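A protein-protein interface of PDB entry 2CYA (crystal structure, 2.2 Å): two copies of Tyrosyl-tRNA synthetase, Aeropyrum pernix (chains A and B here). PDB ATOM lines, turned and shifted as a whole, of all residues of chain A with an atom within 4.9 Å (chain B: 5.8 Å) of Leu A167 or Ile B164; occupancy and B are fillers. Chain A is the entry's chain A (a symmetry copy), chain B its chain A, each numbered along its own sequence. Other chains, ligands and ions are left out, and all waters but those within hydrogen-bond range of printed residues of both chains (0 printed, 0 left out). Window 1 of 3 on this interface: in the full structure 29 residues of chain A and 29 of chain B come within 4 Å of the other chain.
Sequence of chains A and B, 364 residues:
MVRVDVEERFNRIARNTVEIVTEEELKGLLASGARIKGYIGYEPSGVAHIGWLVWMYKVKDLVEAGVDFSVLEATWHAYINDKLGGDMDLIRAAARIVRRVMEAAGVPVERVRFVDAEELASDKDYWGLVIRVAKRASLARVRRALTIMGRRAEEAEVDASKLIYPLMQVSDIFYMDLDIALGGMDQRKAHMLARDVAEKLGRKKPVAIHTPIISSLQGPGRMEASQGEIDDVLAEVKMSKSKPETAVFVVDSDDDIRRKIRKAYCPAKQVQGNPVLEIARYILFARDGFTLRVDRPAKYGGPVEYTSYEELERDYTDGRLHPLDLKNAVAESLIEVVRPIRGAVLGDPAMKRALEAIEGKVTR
The backbone NH (N) of Ser B161 lies within hydrogen-bond range of the backbone carbonyl oxygen (O) of Ala A134.
N of Ala B160 sits at hydrogen-bond distance from O of Ala A134 (3.3 Å).
The backbone carbonyl oxygen (O) of Leu A167 is in hydrogen-bond range of the side-chain hydroxyl (OG) of Ser A171 (2.8 Å).
Ile B164 touches Ala A134.
Ala B160 touches Val A142.
Leu A163 touches Leu B163 (CD2 to CD2, 3.4 Å).
Ile A164 touches Leu B167.
Leu A167 touches Ile B164.
Ile B164 touches two residues of chain A.
Printed residues of chain B within 4 Å of Ala A134: Ala B160, Ser B161 and Ile B164.
Printed residues of chain A within 4 Å of Leu B167: Ile A164.
Ile B80 touches none of the printed residues of chain A.
The nearest residue of chain B that does not touch Leu A167 is Ala B160 (4.2 Å).
The nearest residue of chain A that does not touch Ile B164 is Val A130 (4.3 Å).
Along chain B the printed residues that touch a printed residue of chain A span positions 160 to 167.
Of the 14 printed residues of chain A, 5 touch a printed residue of chain B.
Among the printed residues, 7 pairs touch across the chains.
Among the printed residues, no Asp or Glu carboxylate lies within 4 Å of a Lys or Arg side-chain nitrogen of the other chain.
Leu A163 touches its own counterpart, Leu B163.
Ile A164 touches Leu B167, and with the chains exchanged Leu A167 touches Ile B164.
Of the 7 pairs that touch across the chains among the printed residues, 3 have their exchanged pair printed and touching as well.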
ATOM      1  N   VAL A 130      18.502  -2.058  10.123  1.00  0.00           N
ATOM      2  CA  VAL A 130      17.468  -1.710   9.165  1.00  0.00           C
ATOM      3  C   VAL A 130      17.265  -2.889   8.199  1.00  0.00           C
ATOM      4  O   VAL A 130      16.139  -3.194   7.794  1.00  0.00           O
ATOM      5  CB  VAL A 130      17.842  -0.444   8.386  1.00  0.00           C
ATOM      6  CG1 VAL A 130      16.937  -0.288   7.189  1.00  0.00           C
ATOM      7  CG2 VAL A 130      17.710   0.773   9.310  1.00  0.00           C
ATOM      8  N   VAL A 133      15.621  -5.930  10.051  1.00  0.00           N
ATOM      9  CA  VAL A 133      14.214  -5.650  10.260  1.00  0.00           C
ATOM     10  C   VAL A 133      13.455  -5.838   8.956  1.00  0.00           C
ATOM     11  O   VAL A 133      12.372  -6.400   8.951  1.00  0.00           O
ATOM     12  CB  VAL A 133      13.968  -4.208  10.767  1.00  0.00           C
ATOM     13  CG1 VAL A 133      12.488  -3.910  10.725  1.00  0.00           C
ATOM     14  CG2 VAL A 133      14.494  -4.050  12.202  1.00  0.00           C
ATOM     15  N   ALA A 134      14.017  -5.361   7.849  1.00  0.00           N
ATOM     16  CA  ALA A 134      13.353  -5.494   6.561  1.00  0.00           C
ATOM     17  C   ALA A 134      13.189  -6.959   6.132  1.00  0.00           C
ATOM     18  O   ALA A 134      12.281  -7.285   5.369  1.00  0.00           O
ATOM     19  CB  ALA A 134      14.121  -4.727   5.492  1.00  0.00           C
ATOM     20  N   VAL A 142       4.811  -4.188   5.999  1.00  0.00           N
ATOM     21  CA  VAL A 142       5.388  -2.846   6.028  1.00  0.00           C
ATOM     22  C   VAL A 142       4.463  -1.828   5.390  1.00  0.00           C
ATOM     23  O   VAL A 142       4.439  -0.667   5.782  1.00  0.00           O
ATOM     24  CB  VAL A 142       6.747  -2.786   5.281  1.00  0.00           C
ATOM     25  CG1 VAL A 142       7.225  -1.340   5.183  1.00  0.00           C
ATOM     26  CG2 VAL A 142       7.783  -3.635   6.008  1.00  0.00           C
ATOM     27  N   LEU A 163       8.802   3.405   2.298  1.00  0.00           N
ATOM     28  CA  LEU A 163       8.839   2.087   2.918  1.00  0.00           C
ATOM     29  C   LEU A 163      10.043   2.007   3.846  1.00  0.00           C
ATOM     30  O   LEU A 163      10.030   1.282   4.835  1.00  0.00           O
ATOM     31  CB  LEU A 163       8.930   0.979   1.864  1.00  0.00           C
ATOM     32  CG  LEU A 163       7.600   0.360   1.410  1.00  0.00           C
ATOM     33  CD1 LEU A 163       6.712   1.418   0.753  1.00  0.00           C
ATOM     34  CD2 LEU A 163       7.892  -0.777   0.444  1.00  0.00           C
ATOM     35  N   ILE A 164      11.088   2.756   3.530  1.00  0.00           N
ATOM     36  CA  ILE A 164      12.279   2.752   4.368  1.00  0.00           C
ATOM     37  C   ILE A 164      12.033   3.484   5.697  1.00  0.00           C
ATOM     38  O   ILE A 164      12.570   3.092   6.732  1.00  0.00           O
ATOM     39  CB  ILE A 164      13.468   3.401   3.618  1.00  0.00           C
ATOM     40  CG1 ILE A 164      13.897   2.493   2.461  1.00  0.00           C
ATOM     41  CG2 ILE A 164      14.651   3.584   4.532  1.00  0.00           C
ATOM     42  CD1 ILE A 164      15.116   3.018   1.698  1.00  0.00           C
ATOM     43  N   TYR A 165      11.200   4.523   5.651  1.00  0.00           N
ATOM     44  CA  TYR A 165      10.877   5.353   6.819  1.00  0.00           C
ATOM     45  C   TYR A 165      10.578   4.484   8.044  1.00  0.00           C
ATOM     46  O   TYR A 165      11.316   4.506   9.014  1.00  0.00           O
ATOM     47  CB  TYR A 165       9.689   6.277   6.473  1.00  0.00           C
ATOM     48  CG  TYR A 165       9.339   7.316   7.509  1.00  0.00           C
ATOM     49  CD1 TYR A 165       9.625   8.655   7.297  1.00  0.00           C
ATOM     50  CD2 TYR A 165       8.698   6.958   8.704  1.00  0.00           C
ATOM     51  CE1 TYR A 165       9.278   9.629   8.246  1.00  0.00           C
ATOM     52  CE2 TYR A 165       8.354   7.914   9.658  1.00  0.00           C
ATOM     53  CZ  TYR A 165       8.644   9.247   9.423  1.00  0.00           C
ATOM     54  OH  TYR A 165       8.313  10.197  10.370  1.00  0.00           O
ATOM     55  N   PRO A 166       9.511   3.672   7.991  1.00  0.00           N
ATOM     56  CA  PRO A 166       9.101   2.777   9.092  1.00  0.00           C
ATOM     57  C   PRO A 166      10.217   1.821   9.514  1.00  0.00           C
ATOM     58  O   PRO A 166      10.392   1.519  10.704  1.00  0.00           O
ATOM     59  CB  PRO A 166       7.926   2.003   8.495  1.00  0.00           C
ATOM     60  CG  PRO A 166       7.427   2.883   7.397  1.00  0.00           C
ATOM     61  CD  PRO A 166       8.648   3.492   6.808  1.00  0.00           C
ATOM     62  N   LEU A 167      10.942   1.309   8.529  1.00  0.00           N
ATOM     63  CA  LEU A 167      12.039   0.385   8.780  1.00  0.00           C
ATOM     64  C   LEU A 167      13.056   1.105   9.672  1.00  0.00           C
ATOM     65  O   LEU A 167      13.556   0.544  10.642  1.00  0.00           O
ATOM     66  CB  LEU A 167      12.684  -0.032   7.448  1.00  0.00           C
ATOM     67  CG  LEU A 167      12.329  -1.372   6.771  1.00  0.00           C
ATOM     68  CD1 LEU A 167      10.977  -1.871   7.204  1.00  0.00           C
ATOM     69  CD2 LEU A 167      12.416  -1.214   5.230  1.00  0.00           C
ATOM     70  N   MET A 168      13.335   2.358   9.343  1.00  0.00           N
ATOM     71  CA  MET A 168      14.272   3.163  10.125  1.00  0.00           C
ATOM     72  C   MET A 168      13.694   3.506  11.496  1.00  0.00           C
ATOM     73  O   MET A 168      14.423   3.544  12.484  1.00  0.00           O
ATOM     74  CB  MET A 168      14.613   4.460   9.381  1.00  0.00           C
ATOM     75  CG  MET A 168      15.610   4.248   8.226  1.00  0.00           C
ATOM     76  SD  MET A 168      15.872   5.763   7.303  1.00  0.00           S
ATOM     77  CE  MET A 168      16.702   6.785   8.600  1.00  0.00           C
ATOM     78  N   GLN A 169      12.387   3.767  11.545  1.00  0.00           N
ATOM     79  CA  GLN A 169      11.734   4.110  12.803  1.00  0.00           C
ATOM     80  C   GLN A 169      11.895   2.949  13.778  1.00  0.00           C
ATOM     81  O   GLN A 169      12.368   3.135  14.903  1.00  0.00           O
ATOM     82  CB  GLN A 169      10.253   4.436  12.566  1.00  0.00           C
ATOM     83  CG  GLN A 169       9.551   4.977  13.816  1.00  0.00           C
ATOM     84  CD  GLN A 169       8.369   5.887  13.487  1.00  0.00           C
ATOM     85  OE1 GLN A 169       7.901   5.939  12.341  1.00  0.00           O
ATOM     86  NE2 GLN A 169       7.884   6.614  14.495  1.00  0.00           N
ATOM     87  N   VAL A 170      11.544   1.746  13.335  1.00  0.00           N
ATOM     88  CA  VAL A 170      11.678   0.553  14.170  1.00  0.00           C
ATOM     89  C   VAL A 170      13.156   0.328  14.544  1.00  0.00           C
ATOM     90  O   VAL A 170      13.478  -0.024  15.685  1.00  0.00           O
ATOM     91  CB  VAL A 170      11.150  -0.697  13.422  1.00  0.00           C
ATOM     92  CG1 VAL A 170      11.439  -1.950  14.219  1.00  0.00           C
ATOM     93  CG2 VAL A 170       9.651  -0.560  13.171  1.00  0.00           C
ATOM     94  N   SER A 171      14.061   0.540  13.592  1.00  0.00           N
ATOM     95  CA  SER A 171      15.466   0.324  13.877  1.00  0.00           C
ATOM     96  C   SER A 171      16.016   1.318  14.887  1.00  0.00           C
ATOM     97  O   SER A 171      16.943   0.992  15.618  1.00  0.00           O
ATOM     98  CB  SER A 171      16.292   0.373  12.585  1.00  0.00           C
ATOM     99  OG  SER A 171      15.883  -0.663  11.710  1.00  0.00           O
ATOM    100  N   LEU A 193       4.544  -2.334  14.345  1.00  0.00           N
ATOM    101  CA  LEU A 193       5.468  -3.097  13.518  1.00  0.00           C
ATOM    102  C   LEU A 193       6.689  -3.449  14.364  1.00  0.00           C
ATOM    103  O   LEU A 193       7.234  -4.555  14.263  1.00  0.00           O
ATOM    104  CB  LEU A 193       5.913  -2.249  12.321  1.00  0.00           C
ATOM    105  CG  LEU A 193       6.996  -2.881  11.441  1.00  0.00           C
ATOM    106  CD1 LEU A 193       6.509  -4.243  10.928  1.00  0.00           C
ATOM    107  CD2 LEU A 193       7.330  -1.939  10.298  1.00  0.00           C
ATOM    108  N   ILE B  80      21.359 -10.394   2.351  1.00  0.00           N
ATOM    109  CA  ILE B  80      19.953 -10.143   2.079  1.00  0.00           C
ATOM    110  C   ILE B  80      19.307 -11.348   1.406  1.00  0.00           C
ATOM    111  O   ILE B  80      18.173 -11.698   1.727  1.00  0.00           O
ATOM    112  CB  ILE B  80      19.764  -8.866   1.236  1.00  0.00           C
ATOM    113  CG1 ILE B  80      20.084  -7.646   2.118  1.00  0.00           C
ATOM    114  CG2 ILE B  80      18.340  -8.789   0.691  1.00  0.00           C
ATOM    115  CD1 ILE B  80      20.057  -6.327   1.386  1.00  0.00           C
ATOM    116  N   TRP B 127      24.481   5.573   2.737  1.00  0.00           N
ATOM    117  CA  TRP B 127      23.065   5.408   3.084  1.00  0.00           C
ATOM    118  C   TRP B 127      22.319   6.659   2.684  1.00  0.00           C
ATOM    119  O   TRP B 127      21.162   6.604   2.302  1.00  0.00           O
ATOM    120  CB  TRP B 127      22.907   5.077   4.583  1.00  0.00           C
ATOM    121  CG  TRP B 127      23.542   3.742   4.884  1.00  0.00           C
ATOM    122  CD1 TRP B 127      24.755   3.523   5.498  1.00  0.00           C
ATOM    123  CD2 TRP B 127      23.090   2.462   4.426  1.00  0.00           C
ATOM    124  NE1 TRP B 127      25.084   2.186   5.434  1.00  0.00           N
ATOM    125  CE2 TRP B 127      24.079   1.515   4.780  1.00  0.00           C
ATOM    126  CE3 TRP B 127      21.943   2.023   3.740  1.00  0.00           C
ATOM    127  CZ2 TRP B 127      23.959   0.149   4.473  1.00  0.00           C
ATOM    128  CZ3 TRP B 127      21.825   0.664   3.436  1.00  0.00           C
ATOM    129  CH2 TRP B 127      22.831  -0.255   3.802  1.00  0.00           C
ATOM    130  N   VAL B 130      21.375   5.881  -0.695  1.00  0.00           N
ATOM    131  CA  VAL B 130      20.318   4.888  -0.766  1.00  0.00           C
ATOM    132  C   VAL B 130      18.964   5.586  -0.566  1.00  0.00           C
ATOM    133  O   VAL B 130      17.966   5.236  -1.206  1.00  0.00           O
ATOM    134  CB  VAL B 130      20.514   3.797   0.294  1.00  0.00           C
ATOM    135  CG1 VAL B 130      19.257   2.974   0.426  1.00  0.00           C
ATOM    136  CG2 VAL B 130      21.691   2.902  -0.117  1.00  0.00           C
ATOM    137  N   ALA B 160      10.436  -6.974   2.652  1.00  0.00           N
ATOM    138  CA  ALA B 160      10.965  -5.636   2.387  1.00  0.00           C
ATOM    139  C   ALA B 160      12.444  -5.527   2.017  1.00  0.00           C
ATOM    140  O   ALA B 160      12.825  -4.646   1.251  1.00  0.00           O
ATOM    141  CB  ALA B 160      10.665  -4.719   3.584  1.00  0.00           C
ATOM    142  N   SER B 161      13.279  -6.402   2.558  1.00  0.00           N
ATOM    143  CA  SER B 161      14.697  -6.348   2.247  1.00  0.00           C
ATOM    144  C   SER B 161      14.945  -6.534   0.744  1.00  0.00           C
ATOM    145  O   SER B 161      15.986  -6.127   0.226  1.00  0.00           O
ATOM    146  CB  SER B 161      15.447  -7.407   3.055  1.00  0.00           C
ATOM    147  OG  SER B 161      15.076  -8.707   2.644  1.00  0.00           O
ATOM    148  N   LYS B 162      13.977  -7.117   0.041  1.00  0.00           N
ATOM    149  CA  LYS B 162      14.101  -7.347  -1.398  1.00  0.00           C
ATOM    150  C   LYS B 162      13.985  -6.056  -2.181  1.00  0.00           C
ATOM    151  O   LYS B 162      14.459  -5.970  -3.312  1.00  0.00           O
ATOM    152  CB  LYS B 162      13.033  -8.327  -1.904  1.00  0.00           C
ATOM    153  CG  LYS B 162      13.039  -9.687  -1.232  1.00  0.00           C
ATOM    154  CD  LYS B 162      14.304 -10.462  -1.530  1.00  0.00           C
ATOM    155  CE  LYS B 162      14.223 -11.878  -0.974  1.00  0.00           C
ATOM    156  NZ  LYS B 162      15.371 -12.698  -1.436  1.00  0.00           N
ATOM    157  N   LEU B 163      13.330  -5.056  -1.600  1.00  0.00           N
ATOM    158  CA  LEU B 163      13.196  -3.769  -2.268  1.00  0.00           C
ATOM    159  C   LEU B 163      14.439  -2.933  -1.992  1.00  0.00           C
ATOM    160  O   LEU B 163      14.826  -2.093  -2.797  1.00  0.00           O
ATOM    161  CB  LEU B 163      11.955  -3.015  -1.780  1.00  0.00           C
ATOM    162  CG  LEU B 163      10.676  -3.200  -2.609  1.00  0.00           C
ATOM    163  CD1 LEU B 163      10.240  -4.667  -2.603  1.00  0.00           C
ATOM    164  CD2 LEU B 163       9.585  -2.310  -2.037  1.00  0.00           C
ATOM    165  N   ILE B 164      15.070  -3.165  -0.852  1.00  0.00           N
ATOM    166  CA  ILE B 164      16.276  -2.422  -0.511  1.00  0.00           C
ATOM    167  C   ILE B 164      17.470  -2.862  -1.374  1.00  0.00           C
ATOM    168  O   ILE B 164      18.316  -2.044  -1.728  1.00  0.00           O
ATOM    169  CB  ILE B 164      16.612  -2.601   0.990  1.00  0.00           C
ATOM    170  CG1 ILE B 164      15.554  -1.886   1.838  1.00  0.00           C
ATOM    171  CG2 ILE B 164      17.956  -2.004   1.319  1.00  0.00           C
ATOM    172  CD1 ILE B 164      15.840  -1.948   3.340  1.00  0.00           C
ATOM    173  N   TYR B 165      17.502  -4.148  -1.721  1.00  0.00           N
ATOM    174  CA  TYR B 165      18.584  -4.744  -2.516  1.00  0.00           C
ATOM    175  C   TYR B 165      18.936  -3.858  -3.715  1.00  0.00           C
ATOM    176  O   TYR B 165      20.026  -3.317  -3.786  1.00  0.00           O
ATOM    177  CB  TYR B 165      18.167  -6.163  -2.960  1.00  0.00           C
ATOM    178  CG  TYR B 165      19.235  -6.980  -3.643  1.00  0.00           C
ATOM    179  CD1 TYR B 165      19.839  -8.045  -2.993  1.00  0.00           C
ATOM    180  CD2 TYR B 165      19.632  -6.697  -4.957  1.00  0.00           C
ATOM    181  CE1 TYR B 165      20.814  -8.825  -3.633  1.00  0.00           C
ATOM    182  CE2 TYR B 165      20.604  -7.460  -5.603  1.00  0.00           C
ATOM    183  CZ  TYR B 165      21.190  -8.523  -4.936  1.00  0.00           C
ATOM    184  OH  TYR B 165      22.161  -9.275  -5.569  1.00  0.00           O
ATOM    185  N   PRO B 166      17.994  -3.667  -4.650  1.00  0.00           N
ATOM    186  CA  PRO B 166      18.187  -2.838  -5.858  1.00  0.00           C
ATOM    187  C   PRO B 166      18.611  -1.407  -5.523  1.00  0.00           C
ATOM    188  O   PRO B 166      19.434  -0.798  -6.222  1.00  0.00           O
ATOM    189  CB  PRO B 166      16.809  -2.852  -6.517  1.00  0.00           C
ATOM    190  CG  PRO B 166      16.159  -4.086  -5.984  1.00  0.00           C
ATOM    191  CD  PRO B 166      16.612  -4.179  -4.571  1.00  0.00           C
ATOM    192  N   LEU B 167      18.009  -0.857  -4.477  1.00  0.00           N
ATOM    193  CA  LEU B 167      18.311   0.499  -4.039  1.00  0.00           C
ATOM    194  C   LEU B 167      19.804   0.552  -3.697  1.00  0.00           C
ATOM    195  O   LEU B 167      20.507   1.485  -4.075  1.00  0.00           O
ATOM    196  CB  LEU B 167      17.458   0.852  -2.810  1.00  0.00           C
ATOM    197  CG  LEU B 167      16.166   1.684  -2.943  1.00  0.00           C
ATOM    198  CD1 LEU B 167      15.584   1.586  -4.328  1.00  0.00           C
ATOM    199  CD2 LEU B 167      15.148   1.239  -1.860  1.00  0.00           C
ATOM    200  N   MET B 168      20.277  -0.468  -2.997  1.00  0.00           N
ATOM    201  CA  MET B 168      21.689  -0.549  -2.624  1.00  0.00           C
ATOM    202  C   MET B 168      22.570  -0.799  -3.847  1.00  0.00           C
ATOM    203  O   MET B 168      23.676  -0.271  -3.931  1.00  0.00           O
ATOM    204  CB  MET B 168      21.910  -1.673  -1.604  1.00  0.00           C
ATOM    205  CG  MET B 168      21.455  -1.293  -0.181  1.00  0.00           C
ATOM    206  SD  MET B 168      21.605  -2.681   0.944  1.00  0.00           S
ATOM    207  CE  MET B 168      23.443  -2.880   0.959  1.00  0.00           C
ATOM    208  N   GLN B 169      22.079  -1.614  -4.780  1.00  0.00           N
ATOM    209  CA  GLN B 169      22.838  -1.924  -5.986  1.00  0.00           C
ATOM    210  C   GLN B 169      23.100  -0.633  -6.752  1.00  0.00           C
ATOM    211  O   GLN B 169      24.248  -0.318  -7.079  1.00  0.00           O
ATOM    212  CB  GLN B 169      22.081  -2.941  -6.850  1.00  0.00           C
ATOM    213  CG  GLN B 169      22.902  -3.445  -8.041  1.00  0.00           C
ATOM    214  CD  GLN B 169      22.494  -4.846  -8.494  1.00  0.00           C
ATOM    215  OE1 GLN B 169      21.442  -5.366  -8.096  1.00  0.00           O
ATOM    216  NE2 GLN B 169      23.331  -5.464  -9.329  1.00  0.00           N
